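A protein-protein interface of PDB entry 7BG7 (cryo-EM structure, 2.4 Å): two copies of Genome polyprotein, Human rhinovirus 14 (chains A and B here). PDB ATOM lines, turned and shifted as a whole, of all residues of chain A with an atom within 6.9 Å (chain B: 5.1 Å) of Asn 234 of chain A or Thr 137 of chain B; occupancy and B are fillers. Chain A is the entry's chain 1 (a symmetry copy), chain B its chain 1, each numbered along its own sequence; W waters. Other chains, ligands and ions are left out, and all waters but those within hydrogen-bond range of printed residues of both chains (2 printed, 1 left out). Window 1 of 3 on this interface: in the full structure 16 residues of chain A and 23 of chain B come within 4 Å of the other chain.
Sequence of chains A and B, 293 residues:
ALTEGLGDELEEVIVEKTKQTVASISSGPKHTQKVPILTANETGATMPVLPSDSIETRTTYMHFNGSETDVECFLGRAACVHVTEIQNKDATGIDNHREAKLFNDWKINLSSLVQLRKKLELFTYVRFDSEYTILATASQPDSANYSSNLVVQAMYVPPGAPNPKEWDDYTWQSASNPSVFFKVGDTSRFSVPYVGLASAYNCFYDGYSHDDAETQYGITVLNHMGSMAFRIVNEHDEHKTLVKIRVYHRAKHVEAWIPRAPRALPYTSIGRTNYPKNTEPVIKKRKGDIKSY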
ATOM      1  N   GLN A  87       0.071 -15.843  13.299  1.00  0.00           N
ATOM      2  CA  GLN A  87      -0.555 -15.382  12.077  1.00  0.00           C
ATOM      3  C   GLN A  87       0.076 -16.052  10.874  1.00  0.00           C
ATOM      4  O   GLN A  87       1.261 -16.385  10.867  1.00  0.00           O
ATOM      5  CB  GLN A  87      -0.413 -13.869  11.918  1.00  0.00           C
ATOM      6  CG  GLN A  87      -1.182 -13.061  12.931  1.00  0.00           C
ATOM      7  CD  GLN A  87      -1.112 -11.581  12.643  1.00  0.00           C
ATOM      8  OE1 GLN A  87      -0.453 -11.156  11.698  1.00  0.00           O
ATOM      9  NE2 GLN A  87      -1.790 -10.786  13.457  1.00  0.00           N
ATOM     10  N   ASN A  88      -0.742 -16.220   9.847  1.00  0.00           N
ATOM     11  CA  ASN A  88      -0.293 -16.578   8.514  1.00  0.00           C
ATOM     12  C   ASN A  88      -0.536 -15.370   7.624  1.00  0.00           C
ATOM     13  O   ASN A  88      -1.685 -15.034   7.327  1.00  0.00           O
ATOM     14  CB  ASN A  88      -1.061 -17.791   8.001  1.00  0.00           C
ATOM     15  CG  ASN A  88      -0.523 -18.289   6.686  1.00  0.00           C
ATOM     16  OD1 ASN A  88      -1.284 -18.585   5.770  1.00  0.00           O
ATOM     17  ND2 ASN A  88       0.792 -18.384   6.580  1.00  0.00           N
ATOM     18  N   LYS A  89       0.539 -14.697   7.233  1.00  0.00           N
ATOM     19  CA  LYS A  89       0.423 -13.517   6.394  1.00  0.00           C
ATOM     20  C   LYS A  89       1.680 -13.388   5.550  1.00  0.00           C
ATOM     21  O   LYS A  89       2.697 -14.035   5.804  1.00  0.00           O
ATOM     22  CB  LYS A  89       0.202 -12.254   7.234  1.00  0.00           C
ATOM     23  CG  LYS A  89       1.423 -11.823   8.034  1.00  0.00           C
ATOM     24  CD  LYS A  89       1.127 -10.616   8.903  1.00  0.00           C
ATOM     25  CE  LYS A  89       2.348 -10.184   9.697  1.00  0.00           C
ATOM     26  NZ  LYS A  89       2.045  -9.075  10.638  1.00  0.00           N
ATOM     27  N   SER A 148      -8.639 -20.765   4.989  1.00  0.00           N
ATOM     28  CA  SER A 148      -7.457 -21.487   4.541  1.00  0.00           C
ATOM     29  C   SER A 148      -7.343 -22.840   5.237  1.00  0.00           C
ATOM     30  O   SER A 148      -7.808 -23.029   6.362  1.00  0.00           O
ATOM     31  CB  SER A 148      -6.203 -20.658   4.806  1.00  0.00           C
ATOM     32  OG  SER A 148      -6.231 -19.443   4.081  1.00  0.00           O
ATOM     33  N   ASN A 149      -6.714 -23.791   4.546  1.00  0.00           N
ATOM     34  CA  ASN A 149      -6.402 -25.104   5.109  1.00  0.00           C
ATOM     35  C   ASN A 149      -4.974 -25.066   5.644  1.00  0.00           C
ATOM     36  O   ASN A 149      -4.034 -25.558   5.025  1.00  0.00           O
ATOM     37  CB  ASN A 149      -6.580 -26.204   4.065  1.00  0.00           C
ATOM     38  CG  ASN A 149      -7.899 -26.106   3.333  1.00  0.00           C
ATOM     39  OD1 ASN A 149      -7.954 -26.242   2.115  1.00  0.00           O
ATOM     40  ND2 ASN A 149      -8.974 -25.858   4.074  1.00  0.00           N
ATOM     41  N   LEU A 150      -4.819 -24.469   6.818  1.00  0.00           N
ATOM     42  CA  LEU A 150      -3.501 -24.188   7.360  1.00  0.00           C
ATOM     43  C   LEU A 150      -2.978 -25.379   8.150  1.00  0.00           C
ATOM     44  O   LEU A 150      -3.744 -26.181   8.683  1.00  0.00           O
ATOM     45  CB  LEU A 150      -3.552 -22.954   8.254  1.00  0.00           C
ATOM     46  CG  LEU A 150      -4.046 -21.688   7.563  1.00  0.00           C
ATOM     47  CD1 LEU A 150      -4.099 -20.557   8.561  1.00  0.00           C
ATOM     48  CD2 LEU A 150      -3.165 -21.336   6.382  1.00  0.00           C
ATOM     49  N   VAL A 151      -1.657 -25.495   8.204  1.00  0.00           N
ATOM     50  CA  VAL A 151      -0.979 -26.515   8.992  1.00  0.00           C
ATOM     51  C   VAL A 151      -0.069 -25.825   9.998  1.00  0.00           C
ATOM     52  O   VAL A 151       0.704 -24.936   9.631  1.00  0.00           O
ATOM     53  CB  VAL A 151      -0.177 -27.483   8.104  1.00  0.00           C
ATOM     54  CG1 VAL A 151       0.635 -28.426   8.965  1.00  0.00           C
ATOM     55  CG2 VAL A 151      -1.108 -28.252   7.177  1.00  0.00           C
ATOM     56  N   VAL A 152      -0.167 -26.238  11.250  1.00  0.00           N
ATOM     57  CA  VAL A 152       0.651 -25.720  12.338  1.00  0.00           C
ATOM     58  C   VAL A 152       1.800 -26.683  12.579  1.00  0.00           C
ATOM     59  O   VAL A 152       1.636 -27.900  12.471  1.00  0.00           O
ATOM     60  CB  VAL A 152      -0.187 -25.543  13.618  1.00  0.00           C
ATOM     61  CG1 VAL A 152       0.677 -25.047  14.771  1.00  0.00           C
ATOM     62  CG2 VAL A 152      -1.341 -24.623  13.365  1.00  0.00           C
ATOM     63  N   TRP A 167      10.434 -16.903  10.833  1.00  0.00           N
ATOM     64  CA  TRP A 167       9.332 -17.813  10.557  1.00  0.00           C
ATOM     65  C   TRP A 167       9.800 -19.037   9.782  1.00  0.00           C
ATOM     66  O   TRP A 167       9.323 -20.149  10.025  1.00  0.00           O
ATOM     67  CB  TRP A 167       8.230 -17.081   9.797  1.00  0.00           C
ATOM     68  CG  TRP A 167       7.359 -18.011   9.067  1.00  0.00           C
ATOM     69  CD1 TRP A 167       6.455 -18.866   9.604  1.00  0.00           C
ATOM     70  CD2 TRP A 167       7.310 -18.203   7.656  1.00  0.00           C
ATOM     71  NE1 TRP A 167       5.839 -19.587   8.616  1.00  0.00           N
ATOM     72  CE2 TRP A 167       6.348 -19.198   7.407  1.00  0.00           C
ATOM     73  CE3 TRP A 167       7.986 -17.634   6.579  1.00  0.00           C
ATOM     74  CZ2 TRP A 167       6.042 -19.634   6.124  1.00  0.00           C
ATOM     75  CZ3 TRP A 167       7.680 -18.067   5.306  1.00  0.00           C
ATOM     76  CH2 TRP A 167       6.716 -19.057   5.090  1.00  0.00           C
ATOM     77  N   VAL A 184      -5.022 -26.783  11.380  1.00  0.00           N
ATOM     78  CA  VAL A 184      -5.737 -25.856  12.246  1.00  0.00           C
ATOM     79  C   VAL A 184      -7.186 -26.298  12.350  1.00  0.00           C
ATOM     80  O   VAL A 184      -7.796 -26.735  11.367  1.00  0.00           O
ATOM     81  CB  VAL A 184      -5.621 -24.411  11.736  1.00  0.00           C
ATOM     82  CG1 VAL A 184      -4.183 -23.951  11.804  1.00  0.00           C
ATOM     83  CG2 VAL A 184      -6.161 -24.290  10.328  1.00  0.00           C
ATOM     84  N   ARG A 231       4.478 -22.189  14.600  1.00  0.00           N
ATOM     85  CA  ARG A 231       4.356 -21.385  13.397  1.00  0.00           C
ATOM     86  C   ARG A 231       3.290 -22.016  12.519  1.00  0.00           C
ATOM     87  O   ARG A 231       2.907 -23.167  12.711  1.00  0.00           O
ATOM     88  CB  ARG A 231       5.692 -21.280  12.652  1.00  0.00           C
ATOM     89  CG  ARG A 231       6.201 -22.594  12.095  1.00  0.00           C
ATOM     90  CD  ARG A 231       7.216 -22.412  10.998  1.00  0.00           C
ATOM     91  NE  ARG A 231       7.599 -23.704  10.447  1.00  0.00           N
ATOM     92  CZ  ARG A 231       8.311 -23.878   9.341  1.00  0.00           C
ATOM     93  NH1 ARG A 231       8.734 -22.841   8.635  1.00  0.00           N
ATOM     94  NH2 ARG A 231       8.597 -25.103   8.935  1.00  0.00           N
ATOM     95  N   ILE A 232       2.804 -21.247  11.555  1.00  0.00           N
ATOM     96  CA  ILE A 232       1.955 -21.780  10.499  1.00  0.00           C
ATOM     97  C   ILE A 232       2.841 -22.106   9.309  1.00  0.00           C
ATOM     98  O   ILE A 232       3.500 -21.223   8.750  1.00  0.00           O
ATOM     99  CB  ILE A 232       0.836 -20.802  10.116  1.00  0.00           C
ATOM    100  CG1 ILE A 232      -0.161 -20.676  11.265  1.00  0.00           C
ATOM    101  CG2 ILE A 232       0.145 -21.263   8.842  1.00  0.00           C
ATOM    102  CD1 ILE A 232      -0.585 -19.270  11.556  1.00  0.00           C
ATOM    103  N   VAL A 233       2.865 -23.382   8.929  1.00  0.00           N
ATOM    104  CA  VAL A 233       3.794 -23.836   7.903  1.00  0.00           C
ATOM    105  C   VAL A 233       3.437 -23.239   6.552  1.00  0.00           C
ATOM    106  O   VAL A 233       4.322 -22.955   5.739  1.00  0.00           O
ATOM    107  CB  VAL A 233       3.825 -25.373   7.859  1.00  0.00           C
ATOM    108  CG1 VAL A 233       4.651 -25.849   6.684  1.00  0.00           C
ATOM    109  CG2 VAL A 233       4.371 -25.916   9.163  1.00  0.00           C
ATOM    110  N   ASN A 234       2.153 -23.001   6.304  1.00  0.00           N
ATOM    111  CA  ASN A 234       1.713 -22.541   4.997  1.00  0.00           C
ATOM    112  C   ASN A 234       2.328 -21.202   4.634  1.00  0.00           C
ATOM    113  O   ASN A 234       2.553 -20.342   5.488  1.00  0.00           O
ATOM    114  CB  ASN A 234       0.190 -22.391   4.960  1.00  0.00           C
ATOM    115  CG  ASN A 234      -0.536 -23.670   5.261  1.00  0.00           C
ATOM    116  OD1 ASN A 234      -0.440 -24.206   6.361  1.00  0.00           O
ATOM    117  ND2 ASN A 234      -1.292 -24.161   4.291  1.00  0.00           N
ATOM    118  N   GLU A 235       2.621 -21.042   3.353  1.00  0.00           N
ATOM    119  CA  GLU A 235       2.931 -19.728   2.839  1.00  0.00           C
ATOM    120  C   GLU A 235       1.674 -18.866   2.917  1.00  0.00           C
ATOM    121  O   GLU A 235       0.589 -19.334   3.267  1.00  0.00           O
ATOM    122  CB  GLU A 235       3.459 -19.824   1.410  1.00  0.00           C
ATOM    123  CG  GLU A 235       4.916 -20.228   1.342  1.00  0.00           C
ATOM    124  CD  GLU A 235       5.854 -19.141   1.831  1.00  0.00           C
ATOM    125  OE1 GLU A 235       5.379 -18.022   2.118  1.00  0.00           O
ATOM    126  OE2 GLU A 235       7.067 -19.410   1.942  1.00  0.00           O
ATOM    127  N   HIS A 236       1.819 -17.595   2.583  1.00  0.00           N
ATOM    128  CA  HIS A 236       0.739 -16.644   2.783  1.00  0.00           C
ATOM    129  C   HIS A 236      -0.340 -16.790   1.719  1.00  0.00           C
ATOM    130  O   HIS A 236      -0.070 -17.129   0.564  1.00  0.00           O
ATOM    131  CB  HIS A 236       1.277 -15.218   2.761  1.00  0.00           C
ATOM    132  CG  HIS A 236       1.711 -14.764   1.405  1.00  0.00           C
ATOM    133  ND1 HIS A 236       0.918 -13.982   0.594  1.00  0.00           N
ATOM    134  CD2 HIS A 236       2.847 -14.998   0.706  1.00  0.00           C
ATOM    135  CE1 HIS A 236       1.552 -13.742  -0.538  1.00  0.00           C
ATOM    136  NE2 HIS A 236       2.723 -14.349  -0.497  1.00  0.00           N
ATOM    137  N   ASP A 237      -1.571 -16.515   2.122  1.00  0.00           N
ATOM    138  CA  ASP A 237      -2.676 -16.343   1.201  1.00  0.00           C
ATOM    139  C   ASP A 237      -2.853 -14.851   0.927  1.00  0.00           C
ATOM    140  O   ASP A 237      -2.020 -14.026   1.310  1.00  0.00           O
ATOM    141  CB  ASP A 237      -3.948 -16.956   1.788  1.00  0.00           C
ATOM    142  CG  ASP A 237      -3.848 -18.455   1.977  1.00  0.00           C
ATOM    143  OD1 ASP A 237      -2.742 -19.010   1.829  1.00  0.00           O
ATOM    144  OD2 ASP A 237      -4.881 -19.083   2.296  1.00  0.00           O
ATOM    145  N   LEU B 135       4.727 -33.976   3.260  1.00  0.00           N
ATOM    146  CA  LEU B 135       3.736 -33.015   3.710  1.00  0.00           C
ATOM    147  C   LEU B 135       3.530 -31.985   2.610  1.00  0.00           C
ATOM    148  O   LEU B 135       4.486 -31.341   2.171  1.00  0.00           O
ATOM    149  CB  LEU B 135       4.190 -32.359   5.012  1.00  0.00           C
ATOM    150  CG  LEU B 135       3.363 -31.182   5.525  1.00  0.00           C
ATOM    151  CD1 LEU B 135       2.079 -31.645   6.188  1.00  0.00           C
ATOM    152  CD2 LEU B 135       4.197 -30.354   6.467  1.00  0.00           C
ATOM    153  N   ALA B 136       2.298 -31.865   2.135  1.00  0.00           N
ATOM    154  CA  ALA B 136       1.926 -30.887   1.126  1.00  0.00           C
ATOM    155  C   ALA B 136       1.063 -29.816   1.773  1.00  0.00           C
ATOM    156  O   ALA B 136       0.092 -30.136   2.462  1.00  0.00           O
ATOM    157  CB  ALA B 136       1.174 -31.548  -0.030  1.00  0.00           C
ATOM    158  N   THR B 137       1.427 -28.554   1.571  1.00  0.00           N
ATOM    159  CA  THR B 137       0.676 -27.427   2.109  1.00  0.00           C
ATOM    160  C   THR B 137       0.403 -26.433   0.993  1.00  0.00           C
ATOM    161  O   THR B 137       1.301 -26.112   0.211  1.00  0.00           O
ATOM    162  CB  THR B 137       1.427 -26.742   3.261  1.00  0.00           C
ATOM    163  OG1 THR B 137       2.762 -26.426   2.855  1.00  0.00           O
ATOM    164  CG2 THR B 137       1.479 -27.647   4.478  1.00  0.00           C
ATOM    165  N   ALA B 138      -0.840 -25.980   0.893  1.00  0.00           N
ATOM    166  CA  ALA B 138      -1.262 -25.119  -0.198  1.00  0.00           C
ATOM    167  C   ALA B 138      -1.340 -23.666   0.255  1.00  0.00           C
ATOM    168  O   ALA B 138      -1.700 -23.363   1.394  1.00  0.00           O
ATOM    169  CB  ALA B 138      -2.617 -25.560  -0.747  1.00  0.00           C
ATOM    170  N   SER B 139      -0.999 -22.767  -0.662  1.00  0.00           N
ATOM    171  CA  SER B 139      -1.156 -21.336  -0.474  1.00  0.00           C
ATOM    172  C   SER B 139      -1.688 -20.739  -1.766  1.00  0.00           C
ATOM    173  O   SER B 139      -1.384 -21.223  -2.856  1.00  0.00           O
ATOM    174  CB  SER B 139       0.156 -20.648  -0.081  1.00  0.00           C
ATOM    175  OG  SER B 139       1.098 -20.708  -1.130  1.00  0.00           O
ATOM    176  N   GLY B 185      -2.378 -30.618   2.157  1.00  0.00           N
ATOM    177  CA  GLY B 185      -2.691 -30.379   3.539  1.00  0.00           C
ATOM    178  C   GLY B 185      -2.562 -31.601   4.414  1.00  0.00           C
ATOM    179  O   GLY B 185      -2.458 -31.467   5.634  1.00  0.00           O
ATOM    180  N   LEU B 242      -0.309 -22.457  -5.077  1.00  0.00           N
ATOM    181  CA  LEU B 242       1.079 -22.797  -4.802  1.00  0.00           C
ATOM    182  C   LEU B 242       1.114 -23.893  -3.750  1.00  0.00           C
ATOM    183  O   LEU B 242       0.594 -23.712  -2.648  1.00  0.00           O
ATOM    184  CB  LEU B 242       1.842 -21.570  -4.310  1.00  0.00           C
ATOM    185  CG  LEU B 242       2.613 -20.773  -5.352  1.00  0.00           C
ATOM    186  CD1 LEU B 242       1.720 -20.412  -6.514  1.00  0.00           C
ATOM    187  CD2 LEU B 242       3.167 -19.524  -4.702  1.00  0.00           C
ATOM    188  N   VAL B 243       1.710 -25.029  -4.088  1.00  0.00           N
ATOM    189  CA  VAL B 243       1.817 -26.161  -3.177  1.00  0.00           C
ATOM    190  C   VAL B 243       3.281 -26.348  -2.813  1.00  0.00           C
ATOM    191  O   VAL B 243       4.137 -26.465  -3.694  1.00  0.00           O
ATOM    192  CB  VAL B 243       1.236 -27.446  -3.787  1.00  0.00           C
ATOM    193  CG1 VAL B 243       1.400 -28.599  -2.813  1.00  0.00           C
ATOM    194  CG2 VAL B 243      -0.220 -27.242  -4.165  1.00  0.00           C
ATOM    195  N   LYS B 244       3.566 -26.368  -1.521  1.00  0.00           N
ATOM    196  CA  LYS B 244       4.907 -26.615  -1.017  1.00  0.00           C
ATOM    197  C   LYS B 244       4.982 -28.040  -0.484  1.00  0.00           C
ATOM    198  O   LYS B 244       4.200 -28.426   0.391  1.00  0.00           O
ATOM    199  CB  LYS B 244       5.274 -25.606   0.066  1.00  0.00           C
ATOM    200  CG  LYS B 244       6.687 -25.773   0.580  1.00  0.00           C
ATOM    201  CD  LYS B 244       7.207 -24.523   1.256  1.00  0.00           C
ATOM    202  CE  LYS B 244       7.471 -23.400   0.267  1.00  0.00           C
ATOM    203  NZ  LYS B 244       8.082 -22.225   0.933  1.00  0.00           N
ATOM    204  N   ARG B 246       7.144 -30.870   1.397  1.00  0.00           N
ATOM    205  CA  ARG B 246       8.245 -31.148   2.306  1.00  0.00           C
ATOM    206  C   ARG B 246       8.394 -32.655   2.422  1.00  0.00           C
ATOM    207  O   ARG B 246       7.449 -33.345   2.812  1.00  0.00           O
ATOM    208  CB  ARG B 246       8.004 -30.535   3.683  1.00  0.00           C
ATOM    209  CG  ARG B 246       8.576 -29.164   3.858  1.00  0.00           C
ATOM    210  CD  ARG B 246       8.037 -28.499   5.097  1.00  0.00           C
ATOM    211  NE  ARG B 246       6.938 -27.596   4.794  1.00  0.00           N
ATOM    212  CZ  ARG B 246       7.078 -26.300   4.537  1.00  0.00           C
ATOM    213  NH1 ARG B 246       8.273 -25.732   4.546  1.00  0.00           N
ATOM    214  NH2 ARG B 246       6.010 -25.567   4.273  1.00  0.00           N
HETATM  215  O   HOH W   1       2.375 -23.315   1.582  1.00  0.00           O
HETATM  216  O   HOH W   2      -3.288 -26.887   2.601  1.00  0.00           O
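Hydrophobic or aromatic side chains of chain A that line the printed part of chain B: Val 151 and Val 233. Among the printed residues, 9 pairs touch across the chains.
No position is printed for both chains. Of the 9 pairs that touch across the chains among the printed residues, none has its exchanged pair printed and touching as well.
The side-chain amino group (NZ) of Lys 244 of chain B is in salt-bridge range of the side-chain carboxylate (OE2) of Glu 235 of chain A, 3.2 Å away. The guanidinium group (NH2) of Arg 246 of chain B lies close to the backbone carbonyl oxygen (O) of Val 233 of chain A. The side-chain amide nitrogen (ND2) of Asn 234 of chain A lies within hydrogen-bond range of the backbone carbonyl oxygen (O) of Ala 138 of chain B (3.0 Å).
Water W2 lies within hydrogen-bond range of the backbone carbonyl oxygen (O) of Asn 149 of chain A (2.9 Å) and the backbone NH (N) of Ala 138 of chain B (3.1 Å). Water W1 lies within hydrogen-bond range of N of Glu 235 of chain A and O of Thr 137 of chain B.
Ser 148 of chain A touches none of the printed residues of chain B. Printed residues of chain B within 4 Å of Asn 234 of chain A: Thr 137 and Ala 138. Printed residues of chain B within 4 Å of Asp 237 of chain A: Ser 139. Ala 136 of chain B touches none of the printed residues of chain A. Printed residues of chain A within 4 Å of Gly 185 of chain B: Val 151 (3.8 Å). The nearest printed residue of chain B that does not touch Asn 234 of chain A is Arg 246 of chain B (5.1 Å). The nearest residue of chain A that does not touch Thr 137 of chain B is Val 233 of chain A (4.3 Å).
Among the printed residues, pairs that only touch across the chains: Glu 235 of chain A with Ser 139 of chain B, His 236 of chain A with Ser 139 of chain B, Asp 237 of chain A with Ser 139 of chain B, Val 151 of chain A with Thr 137 of chain B, Val 151 of chain A with Gly 185 of chain B and Asn 234 of chain A with Thr 137 of chain B.
The backbone carbonyl oxygen of Leu 135 of chain B lies within hydrogen-bond range of the backbone NH of Arg 246 of chain B, at 2.8 Å. The side-chain amide oxygen (OD1) of Asn 88 of chain A lies close to the backbone carbonyl oxygen (O) of Glu 235 of chain A. The backbone carbonyl oxygen of Ala 136 of chain B lies within hydrogen-bond range of the backbone NH of Gly 185 of chain B (2.5 Å). The backbone carbonyl oxygen of Val 151 of chain A sits at hydrogen-bond distance from the backbone NH of Val 233 of chain A, at 2.8 Å. The side-chain amide nitrogen (ND2) of Asn 88 of chain A sits at hydrogen-bond distance from the backbone carbonyl oxygen (O) of Asn 234 of chain A, at 2.9 Å. OD1 of Asn 234 of chain A is in hydrogen-bond range of N of Val 151 of chain A.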
